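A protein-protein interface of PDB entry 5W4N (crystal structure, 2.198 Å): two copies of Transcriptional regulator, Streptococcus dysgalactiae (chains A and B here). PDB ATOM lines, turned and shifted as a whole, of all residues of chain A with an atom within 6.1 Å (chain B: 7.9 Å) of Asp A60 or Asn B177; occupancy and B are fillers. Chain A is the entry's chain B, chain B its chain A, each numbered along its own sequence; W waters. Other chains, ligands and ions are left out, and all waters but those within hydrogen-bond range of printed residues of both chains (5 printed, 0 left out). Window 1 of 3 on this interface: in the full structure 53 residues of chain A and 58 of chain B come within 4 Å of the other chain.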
ATOM      1  N   ILE A  57     -31.179  -9.392 -10.098  1.00  0.00           N
ATOM      2  CA  ILE A  57     -29.813  -8.924 -10.296  1.00  0.00           C
ATOM      3  C   ILE A  57     -28.889 -10.090  -9.986  1.00  0.00           C
ATOM      4  O   ILE A  57     -28.949 -10.657  -8.888  1.00  0.00           O
ATOM      5  CB  ILE A  57     -29.483  -7.721  -9.397  1.00  0.00           C
ATOM      6  CG1 ILE A  57     -30.544  -6.630  -9.541  1.00  0.00           C
ATOM      7  CG2 ILE A  57     -28.091  -7.180  -9.711  1.00  0.00           C
ATOM      8  CD1 ILE A  57     -30.421  -5.530  -8.509  1.00  0.00           C
ATOM      9  N   THR A  58     -28.050 -10.462 -10.948  1.00  0.00           N
ATOM     10  CA  THR A  58     -27.042 -11.470 -10.665  1.00  0.00           C
ATOM     11  C   THR A  58     -25.989 -10.889  -9.729  1.00  0.00           C
ATOM     12  O   THR A  58     -25.661  -9.700  -9.787  1.00  0.00           O
ATOM     13  CB  THR A  58     -26.383 -11.969 -11.954  1.00  0.00           C
ATOM     14  OG1 THR A  58     -25.471 -10.980 -12.446  1.00  0.00           O
ATOM     15  CG2 THR A  58     -27.434 -12.258 -13.021  1.00  0.00           C
ATOM     16  N   ILE A  59     -25.471 -11.741  -8.840  1.00  0.00           N
ATOM     17  CA  ILE A  59     -24.435 -11.297  -7.916  1.00  0.00           C
ATOM     18  C   ILE A  59     -23.205 -10.819  -8.677  1.00  0.00           C
ATOM     19  O   ILE A  59     -22.465  -9.961  -8.185  1.00  0.00           O
ATOM     20  CB  ILE A  59     -24.101 -12.427  -6.913  1.00  0.00           C
ATOM     21  CG1 ILE A  59     -22.983 -12.006  -5.955  1.00  0.00           C
ATOM     22  CG2 ILE A  59     -23.736 -13.704  -7.640  1.00  0.00           C
ATOM     23  CD1 ILE A  59     -23.336 -10.812  -5.099  1.00  0.00           C
ATOM     24  N   ASP A  60     -22.988 -11.332  -9.891  1.00  0.00           N
ATOM     25  CA  ASP A  60     -21.899 -10.839 -10.728  1.00  0.00           C
ATOM     26  C   ASP A  60     -22.140  -9.392 -11.150  1.00  0.00           C
ATOM     27  O   ASP A  60     -21.227  -8.560 -11.096  1.00  0.00           O
ATOM     28  CB  ASP A  60     -21.734 -11.741 -11.951  1.00  0.00           C
ATOM     29  CG  ASP A  60     -20.538 -11.362 -12.799  1.00  0.00           C
ATOM     30  OD1 ASP A  60     -19.440 -11.177 -12.232  1.00  0.00           O
ATOM     31  OD2 ASP A  60     -20.692 -11.259 -14.034  1.00  0.00           O
ATOM     32  N   GLU A  61     -23.364  -9.074 -11.576  1.00  0.00           N
ATOM     33  CA  GLU A  61     -23.686  -7.693 -11.922  1.00  0.00           C
ATOM     34  C   GLU A  61     -23.635  -6.793 -10.696  1.00  0.00           C
ATOM     35  O   GLU A  61     -23.234  -5.626 -10.788  1.00  0.00           O
ATOM     36  CB  GLU A  61     -25.064  -7.617 -12.581  1.00  0.00           C
ATOM     37  CG  GLU A  61     -25.128  -8.214 -13.975  1.00  0.00           C
ATOM     38  CD  GLU A  61     -26.546  -8.520 -14.414  1.00  0.00           C
ATOM     39  OE1 GLU A  61     -27.463  -8.449 -13.567  1.00  0.00           O
ATOM     40  OE2 GLU A  61     -26.746  -8.836 -15.605  1.00  0.00           O
ATOM     41  N   PHE A  62     -24.034  -7.319  -9.536  1.00  0.00           N
ATOM     42  CA  PHE A  62     -24.050  -6.511  -8.321  1.00  0.00           C
ATOM     43  C   PHE A  62     -22.639  -6.111  -7.905  1.00  0.00           C
ATOM     44  O   PHE A  62     -22.367  -4.934  -7.644  1.00  0.00           O
ATOM     45  CB  PHE A  62     -24.748  -7.270  -7.194  1.00  0.00           C
ATOM     46  CG  PHE A  62     -24.784  -6.521  -5.892  1.00  0.00           C
ATOM     47  CD1 PHE A  62     -25.552  -5.374  -5.760  1.00  0.00           C
ATOM     48  CD2 PHE A  62     -24.053  -6.960  -4.801  1.00  0.00           C
ATOM     49  CE1 PHE A  62     -25.588  -4.681  -4.565  1.00  0.00           C
ATOM     50  CE2 PHE A  62     -24.085  -6.271  -3.602  1.00  0.00           C
ATOM     51  CZ  PHE A  62     -24.854  -5.129  -3.485  1.00  0.00           C
ATOM     52  N   VAL A  63     -21.722  -7.080  -7.842  1.00  0.00           N
ATOM     53  CA  VAL A  63     -20.380  -6.783  -7.352  1.00  0.00           C
ATOM     54  C   VAL A  63     -19.601  -5.962  -8.372  1.00  0.00           C
ATOM     55  O   VAL A  63     -18.827  -5.072  -8.005  1.00  0.00           O
ATOM     56  CB  VAL A  63     -19.637  -8.079  -6.971  1.00  0.00           C
ATOM     57  CG1 VAL A  63     -20.364  -8.792  -5.842  1.00  0.00           C
ATOM     58  CG2 VAL A  63     -19.478  -8.997  -8.174  1.00  0.00           C
ATOM     59  N   SER A  64     -19.794  -6.238  -9.666  1.00  0.00           N
ATOM     60  CA  SER A  64     -19.086  -5.475 -10.688  1.00  0.00           C
ATOM     61  C   SER A  64     -19.553  -4.025 -10.726  1.00  0.00           C
ATOM     62  O   SER A  64     -18.776  -3.134 -11.091  1.00  0.00           O
ATOM     63  CB  SER A  64     -19.261  -6.130 -12.060  1.00  0.00           C
ATOM     64  OG  SER A  64     -20.616  -6.113 -12.470  1.00  0.00           O
ATOM     65  N   THR A  65     -20.811  -3.771 -10.355  1.00  0.00           N
ATOM     66  CA  THR A  65     -21.281  -2.394 -10.224  1.00  0.00           C
ATOM     67  C   THR A  65     -20.641  -1.709  -9.024  1.00  0.00           C
ATOM     68  O   THR A  65     -20.318  -0.516  -9.081  1.00  0.00           O
ATOM     69  CB  THR A  65     -22.804  -2.365 -10.097  1.00  0.00           C
ATOM     70  OG1 THR A  65     -23.388  -3.172 -11.127  1.00  0.00           O
ATOM     71  CG2 THR A  65     -23.322  -0.942 -10.212  1.00  0.00           C
ATOM     72  N   PHE A  74      -8.254 -12.295 -10.876  1.00  0.00           N
ATOM     73  CA  PHE A  74      -8.568 -11.629 -12.135  1.00  0.00           C
ATOM     74  C   PHE A  74      -7.851 -10.291 -12.244  1.00  0.00           C
ATOM     75  O   PHE A  74      -7.402  -9.909 -13.330  1.00  0.00           O
ATOM     76  CB  PHE A  74     -10.076 -11.430 -12.283  1.00  0.00           C
ATOM     77  CG  PHE A  74     -10.467 -10.799 -13.590  1.00  0.00           C
ATOM     78  CD1 PHE A  74     -10.492 -11.550 -14.754  1.00  0.00           C
ATOM     79  CD2 PHE A  74     -10.787  -9.452 -13.661  1.00  0.00           C
ATOM     80  CE1 PHE A  74     -10.839 -10.974 -15.962  1.00  0.00           C
ATOM     81  CE2 PHE A  74     -11.137  -8.871 -14.866  1.00  0.00           C
ATOM     82  CZ  PHE A  74     -11.163  -9.632 -16.018  1.00  0.00           C
ATOM     83  N   THR A 179     -17.725 -19.107 -19.875  1.00  0.00           N
ATOM     84  CA  THR A 179     -16.400 -18.504 -19.988  1.00  0.00           C
ATOM     85  C   THR A 179     -15.307 -19.553 -19.834  1.00  0.00           C
ATOM     86  O   THR A 179     -14.302 -19.525 -20.556  1.00  0.00           O
ATOM     87  CB  THR A 179     -16.238 -17.397 -18.945  1.00  0.00           C
ATOM     88  OG1 THR A 179     -17.179 -16.350 -19.210  1.00  0.00           O
ATOM     89  CG2 THR A 179     -14.830 -16.823 -18.989  1.00  0.00           C
ATOM     90  N   LEU B  49     -18.097 -12.698  -0.131  1.00  0.00           N
ATOM     91  CA  LEU B  49     -17.322 -12.221  -1.271  1.00  0.00           C
ATOM     92  C   LEU B  49     -15.828 -12.388  -1.030  1.00  0.00           C
ATOM     93  O   LEU B  49     -15.087 -12.791  -1.933  1.00  0.00           O
ATOM     94  CB  LEU B  49     -17.660 -10.757  -1.554  1.00  0.00           C
ATOM     95  CG  LEU B  49     -19.117 -10.472  -1.915  1.00  0.00           C
ATOM     96  CD1 LEU B  49     -19.342  -8.977  -2.115  1.00  0.00           C
ATOM     97  CD2 LEU B  49     -19.520 -11.253  -3.157  1.00  0.00           C
ATOM     98  N   THR B  58     -14.157 -17.031  -9.352  1.00  0.00           N
ATOM     99  CA  THR B  58     -14.795 -15.837  -9.884  1.00  0.00           C
ATOM    100  C   THR B  58     -16.273 -15.816  -9.511  1.00  0.00           C
ATOM    101  O   THR B  58     -16.900 -16.857  -9.293  1.00  0.00           O
ATOM    102  CB  THR B  58     -14.638 -15.763 -11.405  1.00  0.00           C
ATOM    103  OG1 THR B  58     -15.472 -16.747 -12.029  1.00  0.00           O
ATOM    104  CG2 THR B  58     -13.193 -16.002 -11.805  1.00  0.00           C
ATOM    105  N   ILE B  59     -16.828 -14.604  -9.424  1.00  0.00           N
ATOM    106  CA  ILE B  59     -18.251 -14.468  -9.127  1.00  0.00           C
ATOM    107  C   ILE B  59     -19.083 -15.099 -10.231  1.00  0.00           C
ATOM    108  O   ILE B  59     -20.180 -15.616  -9.981  1.00  0.00           O
ATOM    109  CB  ILE B  59     -18.612 -12.985  -8.915  1.00  0.00           C
ATOM    110  CG1 ILE B  59     -17.602 -12.326  -7.975  1.00  0.00           C
ATOM    111  CG2 ILE B  59     -20.016 -12.855  -8.349  1.00  0.00           C
ATOM    112  CD1 ILE B  59     -17.580 -12.933  -6.589  1.00  0.00           C
ATOM    113  N   ASP B  60     -18.576 -15.079 -11.467  1.00  0.00           N
ATOM    114  CA  ASP B  60     -19.240 -15.776 -12.562  1.00  0.00           C
ATOM    115  C   ASP B  60     -19.301 -17.277 -12.301  1.00  0.00           C
ATOM    116  O   ASP B  60     -20.317 -17.923 -12.580  1.00  0.00           O
ATOM    117  CB  ASP B  60     -18.511 -15.487 -13.876  1.00  0.00           C
ATOM    118  CG  ASP B  60     -19.175 -16.143 -15.070  1.00  0.00           C
ATOM    119  OD1 ASP B  60     -20.323 -15.772 -15.390  1.00  0.00           O
ATOM    120  OD2 ASP B  60     -18.546 -17.025 -15.692  1.00  0.00           O
ATOM    121  N   GLU B  61     -18.220 -17.851 -11.765  1.00  0.00           N
ATOM    122  CA  GLU B  61     -18.228 -19.268 -11.412  1.00  0.00           C
ATOM    123  C   GLU B  61     -19.283 -19.562 -10.355  1.00  0.00           C
ATOM    124  O   GLU B  61     -19.970 -20.587 -10.422  1.00  0.00           O
ATOM    125  CB  GLU B  61     -16.846 -19.695 -10.914  1.00  0.00           C
ATOM    126  CG  GLU B  61     -15.830 -19.916 -12.007  1.00  0.00           C
ATOM    127  CD  GLU B  61     -14.509 -20.414 -11.467  1.00  0.00           C
ATOM    128  OE1 GLU B  61     -14.081 -21.513 -11.871  1.00  0.00           O
ATOM    129  OE2 GLU B  61     -13.904 -19.705 -10.637  1.00  0.00           O
ATOM    130  N   PHE B  62     -19.427 -18.667  -9.373  1.00  0.00           N
ATOM    131  CA  PHE B  62     -20.447 -18.846  -8.346  1.00  0.00           C
ATOM    132  C   PHE B  62     -21.849 -18.771  -8.939  1.00  0.00           C
ATOM    133  O   PHE B  62     -22.747 -19.516  -8.529  1.00  0.00           O
ATOM    134  CB  PHE B  62     -20.267 -17.794  -7.250  1.00  0.00           C
ATOM    135  CG  PHE B  62     -21.229 -17.934  -6.105  1.00  0.00           C
ATOM    136  CD1 PHE B  62     -20.947 -18.779  -5.046  1.00  0.00           C
ATOM    137  CD2 PHE B  62     -22.417 -17.222  -6.089  1.00  0.00           C
ATOM    138  CE1 PHE B  62     -21.830 -18.913  -3.992  1.00  0.00           C
ATOM    139  CE2 PHE B  62     -23.308 -17.351  -5.037  1.00  0.00           C
ATOM    140  CZ  PHE B  62     -23.012 -18.197  -3.987  1.00  0.00           C
ATOM    141  N   VAL B  63     -22.055 -17.871  -9.906  1.00  0.00           N
ATOM    142  CA  VAL B  63     -23.359 -17.746 -10.556  1.00  0.00           C
ATOM    143  C   VAL B  63     -23.740 -19.051 -11.243  1.00  0.00           C
ATOM    144  O   VAL B  63     -24.863 -19.549 -11.095  1.00  0.00           O
ATOM    145  CB  VAL B  63     -23.348 -16.572 -11.554  1.00  0.00           C
ATOM    146  CG1 VAL B  63     -24.556 -16.642 -12.479  1.00  0.00           C
ATOM    147  CG2 VAL B  63     -23.313 -15.246 -10.818  1.00  0.00           C
ATOM    148  N   SER B  67     -26.258 -19.774  -8.452  1.00  0.00           N
ATOM    149  CA  SER B  67     -27.392 -18.932  -8.821  1.00  0.00           C
ATOM    150  C   SER B  67     -28.188 -19.517  -9.981  1.00  0.00           C
ATOM    151  O   SER B  67     -29.397 -19.273 -10.086  1.00  0.00           O
ATOM    152  CB  SER B  67     -26.911 -17.524  -9.174  1.00  0.00           C
ATOM    153  OG  SER B  67     -26.271 -16.906  -8.072  1.00  0.00           O
ATOM    154  N   LYS B  68     -27.536 -20.289 -10.855  1.00  0.00           N
ATOM    155  CA  LYS B  68     -28.210 -20.803 -12.043  1.00  0.00           C
ATOM    156  C   LYS B  68     -29.394 -21.694 -11.687  1.00  0.00           C
ATOM    157  O   LYS B  68     -30.393 -21.716 -12.415  1.00  0.00           O
ATOM    158  CB  LYS B  68     -27.217 -21.569 -12.918  1.00  0.00           C
ATOM    159  CG  LYS B  68     -27.235 -21.168 -14.384  1.00  0.00           C
ATOM    160  CD  LYS B  68     -26.520 -19.844 -14.606  1.00  0.00           C
ATOM    161  CE  LYS B  68     -26.328 -19.564 -16.086  1.00  0.00           C
ATOM    162  NZ  LYS B  68     -25.497 -18.351 -16.318  1.00  0.00           N
ATOM    163  N   GLN B 139     -29.411   0.644 -14.542  1.00  0.00           N
ATOM    164  CA  GLN B 139     -28.500  -0.032 -15.452  1.00  0.00           C
ATOM    165  C   GLN B 139     -29.216  -1.224 -16.070  1.00  0.00           C
ATOM    166  O   GLN B 139     -30.182  -1.753 -15.512  1.00  0.00           O
ATOM    167  CB  GLN B 139     -27.216  -0.480 -14.740  1.00  0.00           C
ATOM    168  CG  GLN B 139     -27.410  -1.642 -13.777  1.00  0.00           C
ATOM    169  CD  GLN B 139     -26.133  -2.009 -13.043  1.00  0.00           C
ATOM    170  OE1 GLN B 139     -25.185  -1.226 -12.994  1.00  0.00           O
ATOM    171  NE2 GLN B 139     -26.106  -3.204 -12.463  1.00  0.00           N
ATOM    172  N   TYR B 142     -28.671  -8.478 -17.131  1.00  0.00           N
ATOM    173  CA  TYR B 142     -29.141  -9.619 -17.913  1.00  0.00           C
ATOM    174  C   TYR B 142     -30.664  -9.646 -17.994  1.00  0.00           C
ATOM    175  O   TYR B 142     -31.239  -9.867 -19.065  1.00  0.00           O
ATOM    176  CB  TYR B 142     -28.607 -10.906 -17.282  1.00  0.00           C
ATOM    177  CG  TYR B 142     -28.892 -12.180 -18.043  1.00  0.00           C
ATOM    178  CD1 TYR B 142     -28.246 -12.460 -19.239  1.00  0.00           C
ATOM    179  CD2 TYR B 142     -29.784 -13.119 -17.545  1.00  0.00           C
ATOM    180  CE1 TYR B 142     -28.495 -13.634 -19.928  1.00  0.00           C
ATOM    181  CE2 TYR B 142     -30.039 -14.294 -18.225  1.00  0.00           C
ATOM    182  CZ  TYR B 142     -29.394 -14.546 -19.414  1.00  0.00           C
ATOM    183  OH  TYR B 142     -29.646 -15.716 -20.094  1.00  0.00           O
ATOM    184  N   ALA B 172     -24.754  -3.231 -17.634  1.00  0.00           N
ATOM    185  CA  ALA B 172     -23.853  -3.670 -16.572  1.00  0.00           C
ATOM    186  C   ALA B 172     -22.742  -4.514 -17.182  1.00  0.00           C
ATOM    187  O   ALA B 172     -22.990  -5.614 -17.686  1.00  0.00           O
ATOM    188  CB  ALA B 172     -24.618  -4.454 -15.510  1.00  0.00           C
ATOM    189  N   TYR B 173     -21.516  -4.007 -17.122  1.00  0.00           N
ATOM    190  CA  TYR B 173     -20.382  -4.586 -17.827  1.00  0.00           C
ATOM    191  C   TYR B 173     -19.456  -5.280 -16.838  1.00  0.00           C
ATOM    192  O   TYR B 173     -19.058  -4.686 -15.829  1.00  0.00           O
ATOM    193  CB  TYR B 173     -19.634  -3.497 -18.601  1.00  0.00           C
ATOM    194  CG  TYR B 173     -18.292  -3.912 -19.163  1.00  0.00           C
ATOM    195  CD1 TYR B 173     -18.200  -4.877 -20.158  1.00  0.00           C
ATOM    196  CD2 TYR B 173     -17.118  -3.319 -18.715  1.00  0.00           C
ATOM    197  CE1 TYR B 173     -16.976  -5.250 -20.681  1.00  0.00           C
ATOM    198  CE2 TYR B 173     -15.890  -3.685 -19.232  1.00  0.00           C
ATOM    199  CZ  TYR B 173     -15.824  -4.650 -20.215  1.00  0.00           C
ATOM    200  OH  TYR B 173     -14.605  -5.018 -20.734  1.00  0.00           O
ATOM    201  N   SER B 174     -19.123  -6.535 -17.125  1.00  0.00           N
ATOM    202  CA  SER B 174     -18.164  -7.306 -16.343  1.00  0.00           C
ATOM    203  C   SER B 174     -17.023  -7.717 -17.263  1.00  0.00           C
ATOM    204  O   SER B 174     -17.252  -8.395 -18.269  1.00  0.00           O
ATOM    205  CB  SER B 174     -18.824  -8.535 -15.715  1.00  0.00           C
ATOM    206  OG  SER B 174     -17.873  -9.327 -15.027  1.00  0.00           O
ATOM    207  N   GLU B 175     -15.798  -7.301 -16.925  1.00  0.00           N
ATOM    208  CA  GLU B 175     -14.657  -7.634 -17.777  1.00  0.00           C
ATOM    209  C   GLU B 175     -14.397  -9.134 -17.801  1.00  0.00           C
ATOM    210  O   GLU B 175     -14.030  -9.681 -18.847  1.00  0.00           O
ATOM    211  CB  GLU B 175     -13.404  -6.889 -17.309  1.00  0.00           C
ATOM    212  CG  GLU B 175     -12.719  -6.050 -18.392  1.00  0.00           C
ATOM    213  CD  GLU B 175     -12.033  -6.878 -19.470  1.00  0.00           C
ATOM    214  OE1 GLU B 175     -11.800  -8.086 -19.256  1.00  0.00           O
ATOM    215  OE2 GLU B 175     -11.743  -6.323 -20.549  1.00  0.00           O
ATOM    216  N   GLN B 176     -14.593  -9.819 -16.673  1.00  0.00           N
ATOM    217  CA  GLN B 176     -14.310 -11.247 -16.624  1.00  0.00           C
ATOM    218  C   GLN B 176     -15.294 -12.061 -17.454  1.00  0.00           C
ATOM    219  O   GLN B 176     -14.907 -13.081 -18.034  1.00  0.00           O
ATOM    220  CB  GLN B 176     -14.314 -11.734 -15.172  1.00  0.00           C
ATOM    221  CG  GLN B 176     -13.781 -13.152 -14.985  1.00  0.00           C
ATOM    222  CD  GLN B 176     -14.858 -14.204 -15.163  1.00  0.00           C
ATOM    223  OE1 GLN B 176     -16.048 -13.900 -15.095  1.00  0.00           O
ATOM    224  NE2 GLN B 176     -14.446 -15.446 -15.402  1.00  0.00           N
ATOM    225  N   ASN B 177     -16.552 -11.627 -17.542  1.00  0.00           N
ATOM    226  CA  ASN B 177     -17.621 -12.428 -18.134  1.00  0.00           C
ATOM    227  C   ASN B 177     -17.927 -12.032 -19.577  1.00  0.00           C
ATOM    228  O   ASN B 177     -17.809 -12.859 -20.487  1.00  0.00           O
ATOM    229  CB  ASN B 177     -18.882 -12.314 -17.265  1.00  0.00           C
ATOM    230  CG  ASN B 177     -19.941 -13.327 -17.636  1.00  0.00           C
ATOM    231  OD1 ASN B 177     -19.690 -14.254 -18.406  1.00  0.00           O
ATOM    232  ND2 ASN B 177     -21.135 -13.161 -17.081  1.00  0.00           N
ATOM    233  N   LYS B 178     -18.336 -10.782 -19.797  1.00  0.00           N
ATOM    234  CA  LYS B 178     -18.708 -10.212 -21.094  1.00  0.00           C
ATOM    235  C   LYS B 178     -19.984 -10.811 -21.673  1.00  0.00           C
ATOM    236  O   LYS B 178     -20.255 -10.633 -22.869  1.00  0.00           O
ATOM    237  CB  LYS B 178     -17.578 -10.337 -22.128  1.00  0.00           C
ATOM    238  CG  LYS B 178     -16.196  -9.985 -21.593  1.00  0.00           C
ATOM    239  CD  LYS B 178     -15.563  -8.837 -22.361  1.00  0.00           C
ATOM    240  CE  LYS B 178     -14.052  -8.851 -22.206  1.00  0.00           C
ATOM    241  NZ  LYS B 178     -13.418  -7.640 -22.791  1.00  0.00           N
ATOM    242  N   THR B 179     -20.786 -11.511 -20.867  1.00  0.00           N
ATOM    243  CA  THR B 179     -22.047 -12.057 -21.365  1.00  0.00           C
ATOM    244  C   THR B 179     -23.021 -10.943 -21.733  1.00  0.00           C
ATOM    245  O   THR B 179     -23.631 -10.963 -22.809  1.00  0.00           O
ATOM    246  CB  THR B 179     -22.667 -12.985 -20.320  1.00  0.00           C
ATOM    247  OG1 THR B 179     -21.778 -14.076 -20.056  1.00  0.00           O
ATOM    248  CG2 THR B 179     -23.998 -13.529 -20.818  1.00  0.00           C
ATOM    249  N   ASN B 180     -23.183  -9.961 -20.843  1.00  0.00           N
ATOM    250  CA  ASN B 180     -24.099  -8.855 -21.109  1.00  0.00           C
ATOM    251  C   ASN B 180     -23.653  -8.051 -22.323  1.00  0.00           C
ATOM    252  O   ASN B 180     -24.466  -7.702 -23.185  1.00  0.00           O
ATOM    253  CB  ASN B 180     -24.207  -7.957 -19.876  1.00  0.00           C
ATOM    254  CG  ASN B 180     -25.032  -8.584 -18.771  1.00  0.00           C
ATOM    255  OD1 ASN B 180     -25.725  -9.576 -18.986  1.00  0.00           O
ATOM    256  ND2 ASN B 180     -24.967  -8.001 -17.578  1.00  0.00           N
ATOM    257  N   LYS B 181     -22.353  -7.749 -22.404  1.00  0.00           N
ATOM    258  CA  LYS B 181     -21.836  -6.983 -23.535  1.00  0.00           C
ATOM    259  C   LYS B 181     -22.100  -7.696 -24.856  1.00  0.00           C
ATOM    260  O   LYS B 181     -22.442  -7.057 -25.859  1.00  0.00           O
ATOM    261  CB  LYS B 181     -20.338  -6.733 -23.351  1.00  0.00           C
ATOM    262  CG  LYS B 181     -19.709  -5.876 -24.436  1.00  0.00           C
ATOM    263  CD  LYS B 181     -18.216  -5.701 -24.200  1.00  0.00           C
ATOM    264  CE  LYS B 181     -17.616  -4.706 -25.182  1.00  0.00           C
ATOM    265  NZ  LYS B 181     -16.148  -4.551 -24.987  1.00  0.00           N
ATOM    266  N   THR B 182     -21.955  -9.023 -24.874  1.00  0.00           N
ATOM    267  CA  THR B 182     -22.215  -9.781 -26.093  1.00  0.00           C
ATOM    268  C   THR B 182     -23.690  -9.726 -26.473  1.00  0.00           C
ATOM    269  O   THR B 182     -24.030  -9.567 -27.653  1.00  0.00           O
ATOM    270  CB  THR B 182     -21.759 -11.230 -25.912  1.00  0.00           C
ATOM    271  OG1 THR B 182     -20.355 -11.255 -25.616  1.00  0.00           O
ATOM    272  CG2 THR B 182     -22.021 -12.036 -27.174  1.00  0.00           C
ATOM    273  N   GLU B 218     -12.386  -7.266 -28.666  1.00  0.00           N
ATOM    274  CA  GLU B 218     -13.118  -8.488 -28.376  1.00  0.00           C
ATOM    275  C   GLU B 218     -12.901  -9.485 -29.504  1.00  0.00           C
ATOM    276  O   GLU B 218     -12.458  -9.133 -30.599  1.00  0.00           O
ATOM    277  CB  GLU B 218     -14.625  -8.234 -28.203  1.00  0.00           C
ATOM    278  CG  GLU B 218     -14.981  -7.176 -27.173  1.00  0.00           C
ATOM    279  CD  GLU B 218     -14.788  -7.650 -25.745  1.00  0.00           C
ATOM    280  OE1 GLU B 218     -14.593  -8.867 -25.537  1.00  0.00           O
ATOM    281  OE2 GLU B 218     -14.839  -6.802 -24.830  1.00  0.00           O
HETATM  282  O   HOH W   1     -22.192 -14.009 -14.314  1.00  0.00           O
HETATM  283  O   HOH W   2     -19.519 -17.507 -18.128  1.00  0.00           O
HETATM  284  O   HOH W   3     -29.966  -9.121 -14.167  1.00  0.00           O
HETATM  285  O   HOH W   4     -16.932 -12.820 -12.481  1.00  0.00           O
HETATM  286  O   HOH W   5     -26.882 -14.240  -9.002  1.00  0.00           O
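O of Ile A59 touches CG2 of Ile B59, at 3.8 Å.
Ile A59 touches Val B63.
Asp A60 touches Ile B59 (CA to CG2, 3.6 Å).
OD2 of Asp A60 touches OG of Ser B174, at 3.6 Å.
CG1 of Ile B59 touches CG2 of Val A63 (3.8 Å).
Ser A64 touches Tyr B173 (OG to O, 3.97 Å).
Glu B175 touches Phe A74.
CZ of Phe A74 touches N of Gln B176, at 3.5 Å.
Thr A179 touches Asp B60.
Thr A179 touches Gln B176 (CG2 to NE2, 3.9 Å).
The backbone carbonyl oxygen (O) of Glu A61 is in hydrogen-bond range of the side-chain hydroxyl (OG1) of Thr A65.
The side-chain hydroxyl (OG1) of Thr B179 sits at hydrogen-bond distance from the side-chain amide oxygen (OD1) of Asn B177 (2.7 Å).
The side-chain amide nitrogen (ND2) of Asn B177 sits at hydrogen-bond distance from the side-chain carboxylate (OD1) of Asp B60, 3.2 Å away.
O of Asp A60 lies within hydrogen-bond range of OG of Ser A64 (2.9 Å).
The side-chain hydroxyl (OH) of Tyr B173 sits at hydrogen-bond distance from the side-chain carboxylate (OE2) of Glu B175 (3.2 Å).
O of Ala B172 lies within hydrogen-bond range of ND2 of Asn B180.
Water W3 lies within hydrogen-bond range of the side-chain carboxylate (OE1) of Glu A61 and the backbone NH (N) of Tyr B142.
Water W2 lies within hydrogen-bond range of OD2 of Asp B60, OG1 of Thr A179 and OD1 of Asn B177.
Water W1 lies within hydrogen-bond range of OD1 of Asp B60 (2.8 Å), ND2 of Asn B177 (3.1 Å) and OD2 of Asp A60 (3.1 Å).
Water W5 bridges N of Ile A59 (2.9 Å) and OG of Ser B67 (2.9 Å).
Water W4 lies within hydrogen-bond range of OE1 of Gln B176 (3.0 Å), N of Asp B60 (3.0 Å) and OD1 of Asp A60 (3.0 Å).
Ile A59 touches its own counterpart, Ile B59.
Ile A59 touches Val B63, and with the chains exchanged Val A63 touches Ile B59.
Asp A60 touches Ile B59, but with the chains exchanged Ile A59 does not touch Asp B60 (6.6 Å).
Thr A179 touches Asp B60, but with the chains exchanged Asp A60 does not touch Thr B179 (6.7 Å).
7 positions are printed for both chains.
Of the 16 pairs that touch across the chains among the printed residues, 3 have their exchanged pair printed and touching as well.
Hydrophobic or aromatic side chains of chain B that line the printed part of chain A: Leu B49, Ile B59, Val B63 and Tyr B142.
Of the 11 printed residues of chain A, 8 touch a printed residue of chain B.
Among the printed residues, no Asp or Glu carboxylate lies within 4 Å of a Lys or Arg side-chain nitrogen of the other chain.
The side-chain amide nitrogen of Asn B180 sits at hydrogen-bond distance from the side-chain carboxylate of Glu A61, at 2.8 Å.
N of Tyr B142 is in hydrogen-bond range of OE2 of Glu A61, 2.5 Å away.
OD1 of Asn B177 lies within hydrogen-bond range of OG1 of Thr A179, 3.4 Å away.
NE2 of Gln B139 is in hydrogen-bond range of OG1 of Thr A65, at 3.0 Å.
Thr A58 touches none of the printed residues of chain B.
Of the printed residues of chain B, Asp A60 touches Ile B59 (3.6 Å), Ser B174 (3.6 Å) and Asn B177 (3.6 Å).
Of the printed residues of chain A, Leu B49 touches Val A63 (3.7 Å).
Of the printed residues of chain A, Gln B139 touches Thr A65 (3.0 Å).
Printed residues of chain A within 4 Å of Ser B174: Asp A60 (3.6 Å).
Printed residues of chain A within 4 Å of Asn B177: Asp A60 (3.6 Å) and Thr A179 (3.4 Å).
Glu B218 touches none of the printed residues of chain A.
The nearest printed residue of chain B that does not touch Asp A60 is Val B63 (4.01 Å).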
